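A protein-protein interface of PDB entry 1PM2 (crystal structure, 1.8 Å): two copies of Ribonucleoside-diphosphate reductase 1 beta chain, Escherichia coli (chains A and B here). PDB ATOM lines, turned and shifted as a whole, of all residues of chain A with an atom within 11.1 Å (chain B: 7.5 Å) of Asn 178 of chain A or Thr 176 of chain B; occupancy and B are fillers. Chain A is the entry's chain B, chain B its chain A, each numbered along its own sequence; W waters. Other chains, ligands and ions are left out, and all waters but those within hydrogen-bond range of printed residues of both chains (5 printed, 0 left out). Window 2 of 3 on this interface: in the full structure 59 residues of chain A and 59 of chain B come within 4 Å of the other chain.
ND2 of Asn 178 of chain A sits at hydrogen-bond distance from ND1 of His 175 of chain B, at 3.0 Å.
N of Asn 178 of chain A sits at hydrogen-bond distance from O of Thr 176 of chain B.
A ring nitrogen (ND1) of His 175 of chain A sits at hydrogen-bond distance from the side-chain amide nitrogen (ND2) of Asn 178 of chain B, at 3.1 Å.
The backbone NH (N) of Asn 178 of chain B sits at hydrogen-bond distance from the backbone carbonyl oxygen (O) of Thr 176 of chain A, at 2.8 Å.
N of His 175 of chain B is in hydrogen-bond range of O of Val 182 of chain B, 2.7 Å away.
O of His 175 of chain A is in hydrogen-bond range of N of Val 182 of chain A (2.7 Å).
CE2 of Tyr 166 of chain A touches CD2 of Leu 169 of chain B, at 3.4 Å.
Leu 170 of chain A touches Val 177 of chain B (CD2 to CG1, 3.7 Å).
Thr 176 of chain B touches Thr 176 of chain A.
Val 177 of chain B touches Thr 176 of chain A (CA to O, 3.6 Å).
Val 177 of chain A touches Leu 170 of chain B (CG1 to CD2, 3.6 Å).
CA of Val 177 of chain A touches O of Thr 176 of chain B, at 3.4 Å.
Of the printed residues of chain B, Thr 176 of chain A touches Thr 176, Val 177 and Asn 178.
Of the printed residues of chain B, Val 177 of chain A touches Leu 170 and Thr 176.
Of chain B, only His 175 and Thr 176 come within 4 Å of Asn 178 of chain A.
Lys 180 of chain A touches none of the printed residues of chain B.
His 175 of chain B touches one residue of chain A.
Of the printed residues of chain A, Thr 176 of chain B touches Thr 176 (3.6 Å), Val 177 (3.4 Å) and Asn 178 (2.9 Å).
No residue of chain A comes within 4 Å of Thr 181 of chain B.
No residue of chain A comes within 4 Å of Val 182 of chain B.
Thr 183 of chain B touches none of the printed residues of chain A.
Hydrophobic or aromatic side chains of chain B within 4 Å of the printed part of chain A: Leu 169, Leu 170, His 175 and Val 177.
Among the printed residues, no Asp or Glu carboxylate lies within 4 Å of a Lys or Arg side-chain nitrogen of the other chain.
Leu 170 of chain A touches Val 177 of chain B, and with the chains exchanged Val 177 of chain A touches Leu 170 of chain B.
Thr 176 of chain B touches its own counterpart, Thr 176 of chain A.
Thr 176 of chain A touches Val 177 of chain B, and with the chains exchanged Val 177 of chain A touches Thr 176 of chain B.
Thr 176 of chain A touches Asn 178 of chain B, and with the chains exchanged Asn 178 of chain A touches Thr 176 of chain B.
Positions printed for both chains: 170, 174, 175, 176, 177, 178, 179, 180, 181 and 182.
Of the 10 pairs that touch across the chains among the printed residues, 9 have their exchanged pair printed and touching as well.
Water W4 lies within hydrogen-bond range of OG1 of Thr 176 of chain A (2.5 Å) and OD1 of Asn 178 of chain B (3.4 Å).
Water W3 lies within hydrogen-bond range of ND1 of His 175 of chain A (2.7 Å), OD1 of Asn 178 of chain B (3.3 Å) and O of Thr 174 of chain A (3.4 Å).
Water W2 lies within hydrogen-bond range of OG1 of Thr 176 of chain A (2.8 Å), O of Thr 176 of chain B (3.0 Å), N of Gly 179 of chain B (3.1 Å) and N of Asn 178 of chain B (3.2 Å).
Water W5 lies within hydrogen-bond range of O of Leu 170 of chain A and ND2 of Asn 178 of chain B.
Water W1 bridges OD1 of Asn 178 of chain A and OG1 of Thr 176 of chain B.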
ATOM      1  N   TYR A 166     -27.205  14.050  -7.633  1.00  0.00           N
ATOM      2  CA  TYR A 166     -26.985  15.464  -7.362  1.00  0.00           C
ATOM      3  C   TYR A 166     -27.239  15.758  -5.889  1.00  0.00           C
ATOM      4  O   TYR A 166     -26.495  16.509  -5.256  1.00  0.00           O
ATOM      5  CB  TYR A 166     -27.911  16.322  -8.223  1.00  0.00           C
ATOM      6  CG  TYR A 166     -27.348  16.622  -9.590  1.00  0.00           C
ATOM      7  CD1 TYR A 166     -26.218  17.425  -9.733  1.00  0.00           C
ATOM      8  CD2 TYR A 166     -27.950  16.116 -10.741  1.00  0.00           C
ATOM      9  CE1 TYR A 166     -25.702  17.721 -10.989  1.00  0.00           C
ATOM     10  CE2 TYR A 166     -27.443  16.406 -12.004  1.00  0.00           C
ATOM     11  CZ  TYR A 166     -26.320  17.212 -12.119  1.00  0.00           C
ATOM     12  OH  TYR A 166     -25.826  17.522 -13.367  1.00  0.00           O
ATOM     13  N   LEU A 170     -24.198  17.225  -3.890  1.00  0.00           N
ATOM     14  CA  LEU A 170     -24.272  18.648  -3.575  1.00  0.00           C
ATOM     15  C   LEU A 170     -25.234  19.060  -2.465  1.00  0.00           C
ATOM     16  O   LEU A 170     -25.072  20.126  -1.866  1.00  0.00           O
ATOM     17  CB  LEU A 170     -24.624  19.423  -4.847  1.00  0.00           C
ATOM     18  CG  LEU A 170     -23.792  19.097  -6.091  1.00  0.00           C
ATOM     19  CD1 LEU A 170     -24.273  19.939  -7.265  1.00  0.00           C
ATOM     20  CD2 LEU A 170     -22.320  19.364  -5.809  1.00  0.00           C
ATOM     21  N   THR A 174     -29.009  26.035  -4.400  1.00  0.00           N
ATOM     22  CA  THR A 174     -28.826  26.516  -5.761  1.00  0.00           C
ATOM     23  C   THR A 174     -27.327  26.457  -6.018  1.00  0.00           C
ATOM     24  O   THR A 174     -26.552  27.186  -5.401  1.00  0.00           O
ATOM     25  CB  THR A 174     -29.330  27.958  -5.906  1.00  0.00           C
ATOM     26  OG1 THR A 174     -30.709  28.015  -5.519  1.00  0.00           O
ATOM     27  CG2 THR A 174     -29.195  28.431  -7.346  1.00  0.00           C
ATOM     28  N   HIS A 175     -26.928  25.576  -6.928  1.00  0.00           N
ATOM     29  CA  HIS A 175     -25.519  25.380  -7.238  1.00  0.00           C
ATOM     30  C   HIS A 175     -25.178  25.819  -8.653  1.00  0.00           C
ATOM     31  O   HIS A 175     -26.056  26.199  -9.425  1.00  0.00           O
ATOM     32  CB  HIS A 175     -25.177  23.898  -7.079  1.00  0.00           C
ATOM     33  CG  HIS A 175     -25.668  23.300  -5.797  1.00  0.00           C
ATOM     34  ND1 HIS A 175     -25.112  23.603  -4.573  1.00  0.00           N
ATOM     35  CD2 HIS A 175     -26.679  22.433  -5.547  1.00  0.00           C
ATOM     36  CE1 HIS A 175     -25.759  22.949  -3.624  1.00  0.00           C
ATOM     37  NE2 HIS A 175     -26.715  22.232  -4.188  1.00  0.00           N
ATOM     38  N   THR A 176     -23.891  25.769  -8.979  1.00  0.00           N
ATOM     39  CA  THR A 176     -23.424  26.112 -10.312  1.00  0.00           C
ATOM     40  C   THR A 176     -22.471  25.015 -10.759  1.00  0.00           C
ATOM     41  O   THR A 176     -21.615  24.565  -9.994  1.00  0.00           O
ATOM     42  CB  THR A 176     -22.689  27.474 -10.352  1.00  0.00           C
ATOM     43  OG1 THR A 176     -21.575  27.453  -9.453  1.00  0.00           O
ATOM     44  CG2 THR A 176     -23.636  28.594  -9.963  1.00  0.00           C
ATOM     45  N   VAL A 177     -22.646  24.571 -11.995  1.00  0.00           N
ATOM     46  CA  VAL A 177     -21.810  23.532 -12.571  1.00  0.00           C
ATOM     47  C   VAL A 177     -21.442  23.960 -13.982  1.00  0.00           C
ATOM     48  O   VAL A 177     -22.303  24.048 -14.854  1.00  0.00           O
ATOM     49  CB  VAL A 177     -22.562  22.176 -12.624  1.00  0.00           C
ATOM     50  CG1 VAL A 177     -21.735  21.145 -13.370  1.00  0.00           C
ATOM     51  CG2 VAL A 177     -22.858  21.695 -11.211  1.00  0.00           C
ATOM     52  N   ASN A 178     -20.159  24.233 -14.193  1.00  0.00           N
ATOM     53  CA  ASN A 178     -19.659  24.651 -15.493  1.00  0.00           C
ATOM     54  C   ASN A 178     -20.472  25.775 -16.126  1.00  0.00           C
ATOM     55  O   ASN A 178     -20.879  25.682 -17.286  1.00  0.00           O
ATOM     56  CB  ASN A 178     -19.595  23.452 -16.446  1.00  0.00           C
ATOM     57  CG  ASN A 178     -18.629  22.384 -15.969  1.00  0.00           C
ATOM     58  OD1 ASN A 178     -17.560  22.691 -15.435  1.00  0.00           O
ATOM     59  ND2 ASN A 178     -18.992  21.122 -16.171  1.00  0.00           N
ATOM     60  N   GLY A 179     -20.712  26.832 -15.354  1.00  0.00           N
ATOM     61  CA  GLY A 179     -21.441  27.979 -15.867  1.00  0.00           C
ATOM     62  C   GLY A 179     -22.951  27.878 -15.856  1.00  0.00           C
ATOM     63  O   GLY A 179     -23.640  28.836 -16.206  1.00  0.00           O
ATOM     64  N   LYS A 180     -23.469  26.724 -15.457  1.00  0.00           N
ATOM     65  CA  LYS A 180     -24.912  26.519 -15.406  1.00  0.00           C
ATOM     66  C   LYS A 180     -25.414  26.427 -13.977  1.00  0.00           C
ATOM     67  O   LYS A 180     -24.745  25.866 -13.111  1.00  0.00           O
ATOM     68  CB  LYS A 180     -25.296  25.237 -16.146  1.00  0.00           C
ATOM     69  CG  LYS A 180     -25.226  25.328 -17.654  1.00  0.00           C
ATOM     70  CD  LYS A 180     -25.577  23.992 -18.293  1.00  0.00           C
ATOM     71  CE  LYS A 180     -25.650  24.103 -19.806  1.00  0.00           C
ATOM     72  NZ  LYS A 180     -26.753  25.013 -20.231  1.00  0.00           N
ATOM     73  N   THR A 181     -26.600  26.977 -13.738  1.00  0.00           N
ATOM     74  CA  THR A 181     -27.205  26.927 -12.416  1.00  0.00           C
ATOM     75  C   THR A 181     -27.900  25.576 -12.276  1.00  0.00           C
ATOM     76  O   THR A 181     -28.644  25.154 -13.162  1.00  0.00           O
ATOM     77  CB  THR A 181     -28.253  28.046 -12.226  1.00  0.00           C
ATOM     78  OG1 THR A 181     -27.625  29.325 -12.380  1.00  0.00           O
ATOM     79  CG2 THR A 181     -28.872  27.964 -10.837  1.00  0.00           C
ATOM     80  N   VAL A 182     -27.639  24.896 -11.166  1.00  0.00           N
ATOM     81  CA  VAL A 182     -28.233  23.593 -10.903  1.00  0.00           C
ATOM     82  C   VAL A 182     -28.943  23.669  -9.562  1.00  0.00           C
ATOM     83  O   VAL A 182     -28.311  23.871  -8.525  1.00  0.00           O
ATOM     84  CB  VAL A 182     -27.159  22.488 -10.840  1.00  0.00           C
ATOM     85  CG1 VAL A 182     -27.801  21.155 -10.497  1.00  0.00           C
ATOM     86  CG2 VAL A 182     -26.426  22.402 -12.169  1.00  0.00           C
ATOM     87  N   LEU B 169     -22.617  11.959 -13.861  1.00  0.00           N
ATOM     88  CA  LEU B 169     -23.217  13.286 -13.958  1.00  0.00           C
ATOM     89  C   LEU B 169     -22.462  14.276 -14.844  1.00  0.00           C
ATOM     90  O   LEU B 169     -23.068  14.962 -15.667  1.00  0.00           O
ATOM     91  CB  LEU B 169     -23.368  13.909 -12.566  1.00  0.00           C
ATOM     92  CG  LEU B 169     -24.382  13.309 -11.587  1.00  0.00           C
ATOM     93  CD1 LEU B 169     -24.291  14.040 -10.254  1.00  0.00           C
ATOM     94  CD2 LEU B 169     -25.786  13.424 -12.160  1.00  0.00           C
ATOM     95  N   LEU B 170     -21.144  14.340 -14.678  1.00  0.00           N
ATOM     96  CA  LEU B 170     -20.323  15.296 -15.420  1.00  0.00           C
ATOM     97  C   LEU B 170     -19.508  14.761 -16.587  1.00  0.00           C
ATOM     98  O   LEU B 170     -19.209  15.501 -17.528  1.00  0.00           O
ATOM     99  CB  LEU B 170     -19.371  15.997 -14.451  1.00  0.00           C
ATOM    100  CG  LEU B 170     -20.006  16.568 -13.182  1.00  0.00           C
ATOM    101  CD1 LEU B 170     -18.933  17.211 -12.327  1.00  0.00           C
ATOM    102  CD2 LEU B 170     -21.083  17.578 -13.555  1.00  0.00           C
ATOM    103  N   THR B 174     -12.215  18.280 -16.599  1.00  0.00           N
ATOM    104  CA  THR B 174     -12.000  19.100 -15.416  1.00  0.00           C
ATOM    105  C   THR B 174     -13.180  20.054 -15.371  1.00  0.00           C
ATOM    106  O   THR B 174     -13.431  20.791 -16.326  1.00  0.00           O
ATOM    107  CB  THR B 174     -10.677  19.879 -15.502  1.00  0.00           C
ATOM    108  OG1 THR B 174      -9.592  18.952 -15.645  1.00  0.00           O
ATOM    109  CG2 THR B 174     -10.460  20.691 -14.240  1.00  0.00           C
ATOM    110  N   HIS B 175     -13.902  20.035 -14.258  1.00  0.00           N
ATOM    111  CA  HIS B 175     -15.101  20.848 -14.110  1.00  0.00           C
ATOM    112  C   HIS B 175     -15.031  21.869 -12.993  1.00  0.00           C
ATOM    113  O   HIS B 175     -14.107  21.864 -12.179  1.00  0.00           O
ATOM    114  CB  HIS B 175     -16.288  19.923 -13.853  1.00  0.00           C
ATOM    115  CG  HIS B 175     -16.384  18.787 -14.819  1.00  0.00           C
ATOM    116  ND1 HIS B 175     -17.001  18.903 -16.045  1.00  0.00           N
ATOM    117  CD2 HIS B 175     -15.918  17.517 -14.750  1.00  0.00           C
ATOM    118  CE1 HIS B 175     -16.914  17.753 -16.689  1.00  0.00           C
ATOM    119  NE2 HIS B 175     -16.261  16.895 -15.926  1.00  0.00           N
ATOM    120  N   THR B 176     -16.034  22.739 -12.962  1.00  0.00           N
ATOM    121  CA  THR B 176     -16.146  23.768 -11.939  1.00  0.00           C
ATOM    122  C   THR B 176     -17.491  23.565 -11.248  1.00  0.00           C
ATOM    123  O   THR B 176     -18.548  23.831 -11.825  1.00  0.00           O
ATOM    124  CB  THR B 176     -16.074  25.169 -12.561  1.00  0.00           C
ATOM    125  OG1 THR B 176     -14.852  25.292 -13.302  1.00  0.00           O
ATOM    126  CG2 THR B 176     -16.113  26.236 -11.476  1.00  0.00           C
ATOM    127  N   VAL B 177     -17.434  23.074 -10.014  1.00  0.00           N
ATOM    128  CA  VAL B 177     -18.626  22.790  -9.221  1.00  0.00           C
ATOM    129  C   VAL B 177     -18.648  23.713  -8.008  1.00  0.00           C
ATOM    130  O   VAL B 177     -17.813  23.596  -7.110  1.00  0.00           O
ATOM    131  CB  VAL B 177     -18.624  21.314  -8.754  1.00  0.00           C
ATOM    132  CG1 VAL B 177     -19.908  20.992  -8.013  1.00  0.00           C
ATOM    133  CG2 VAL B 177     -18.451  20.393  -9.956  1.00  0.00           C
ATOM    134  N   ASN B 178     -19.611  24.628  -7.992  1.00  0.00           N
ATOM    135  CA  ASN B 178     -19.737  25.609  -6.919  1.00  0.00           C
ATOM    136  C   ASN B 178     -18.425  26.352  -6.699  1.00  0.00           C
ATOM    137  O   ASN B 178     -17.998  26.563  -5.563  1.00  0.00           O
ATOM    138  CB  ASN B 178     -20.191  24.951  -5.612  1.00  0.00           C
ATOM    139  CG  ASN B 178     -21.649  24.548  -5.647  1.00  0.00           C
ATOM    140  OD1 ASN B 178     -22.458  25.175  -6.332  1.00  0.00           O
ATOM    141  ND2 ASN B 178     -21.998  23.510  -4.895  1.00  0.00           N
ATOM    142  N   GLY B 179     -17.788  26.739  -7.801  1.00  0.00           N
ATOM    143  CA  GLY B 179     -16.538  27.473  -7.720  1.00  0.00           C
ATOM    144  C   GLY B 179     -15.309  26.636  -7.419  1.00  0.00           C
ATOM    145  O   GLY B 179     -14.202  27.169  -7.312  1.00  0.00           O
ATOM    146  N   LYS B 180     -15.493  25.329  -7.279  1.00  0.00           N
ATOM    147  CA  LYS B 180     -14.378  24.435  -6.991  1.00  0.00           C
ATOM    148  C   LYS B 180     -14.013  23.638  -8.235  1.00  0.00           C
ATOM    149  O   LYS B 180     -14.881  23.266  -9.023  1.00  0.00           O
ATOM    150  CB  LYS B 180     -14.747  23.474  -5.859  1.00  0.00           C
ATOM    151  CG  LYS B 180     -15.146  24.162  -4.563  1.00  0.00           C
ATOM    152  CD  LYS B 180     -13.995  24.972  -3.988  1.00  0.00           C
ATOM    153  CE  LYS B 180     -14.410  25.687  -2.710  1.00  0.00           C
ATOM    154  NZ  LYS B 180     -14.918  24.738  -1.680  1.00  0.00           N
ATOM    155  N   THR B 181     -12.724  23.380  -8.410  1.00  0.00           N
ATOM    156  CA  THR B 181     -12.254  22.625  -9.559  1.00  0.00           C
ATOM    157  C   THR B 181     -12.314  21.136  -9.243  1.00  0.00           C
ATOM    158  O   THR B 181     -11.617  20.647  -8.355  1.00  0.00           O
ATOM    159  CB  THR B 181     -10.807  23.011  -9.918  1.00  0.00           C
ATOM    160  OG1 THR B 181     -10.726  24.431 -10.103  1.00  0.00           O
ATOM    161  CG2 THR B 181     -10.377  22.322 -11.201  1.00  0.00           C
ATOM    162  N   VAL B 182     -13.159  20.419  -9.974  1.00  0.00           N
ATOM    163  CA  VAL B 182     -13.321  18.986  -9.771  1.00  0.00           C
ATOM    164  C   VAL B 182     -12.848  18.222 -10.999  1.00  0.00           C
ATOM    165  O   VAL B 182     -13.346  18.434 -12.106  1.00  0.00           O
ATOM    166  CB  VAL B 182     -14.798  18.625  -9.500  1.00  0.00           C
ATOM    167  CG1 VAL B 182     -14.952  17.116  -9.347  1.00  0.00           C
ATOM    168  CG2 VAL B 182     -15.286  19.336  -8.245  1.00  0.00           C
ATOM    169  N   THR B 183     -11.875  17.342 -10.803  1.00  0.00           N
ATOM    170  CA  THR B 183     -11.351  16.545 -11.903  1.00  0.00           C
ATOM    171  C   THR B 183     -12.017  15.172 -11.933  1.00  0.00           C
ATOM    172  O   THR B 183     -12.091  14.487 -10.914  1.00  0.00           O
ATOM    173  CB  THR B 183      -9.828  16.344 -11.775  1.00  0.00           C
ATOM    174  OG1 THR B 183      -9.179  17.622 -11.721  1.00  0.00           O
ATOM    175  CG2 THR B 183      -9.296  15.566 -12.969  1.00  0.00           C
HETATM  176  O   HOH W   1     -15.448  24.502 -15.977  1.00  0.00           O
HETATM  177  O   HOH W   2     -19.223  26.504 -10.570  1.00  0.00           O
HETATM  178  O   HOH W   3     -24.060  25.868  -3.483  1.00  0.00           O
HETATM  179  O   HOH W   4     -21.761  28.444  -7.165  1.00  0.00           O
HETATM  180  O   HOH W   5     -22.717  21.604  -2.376  1.00  0.00           O
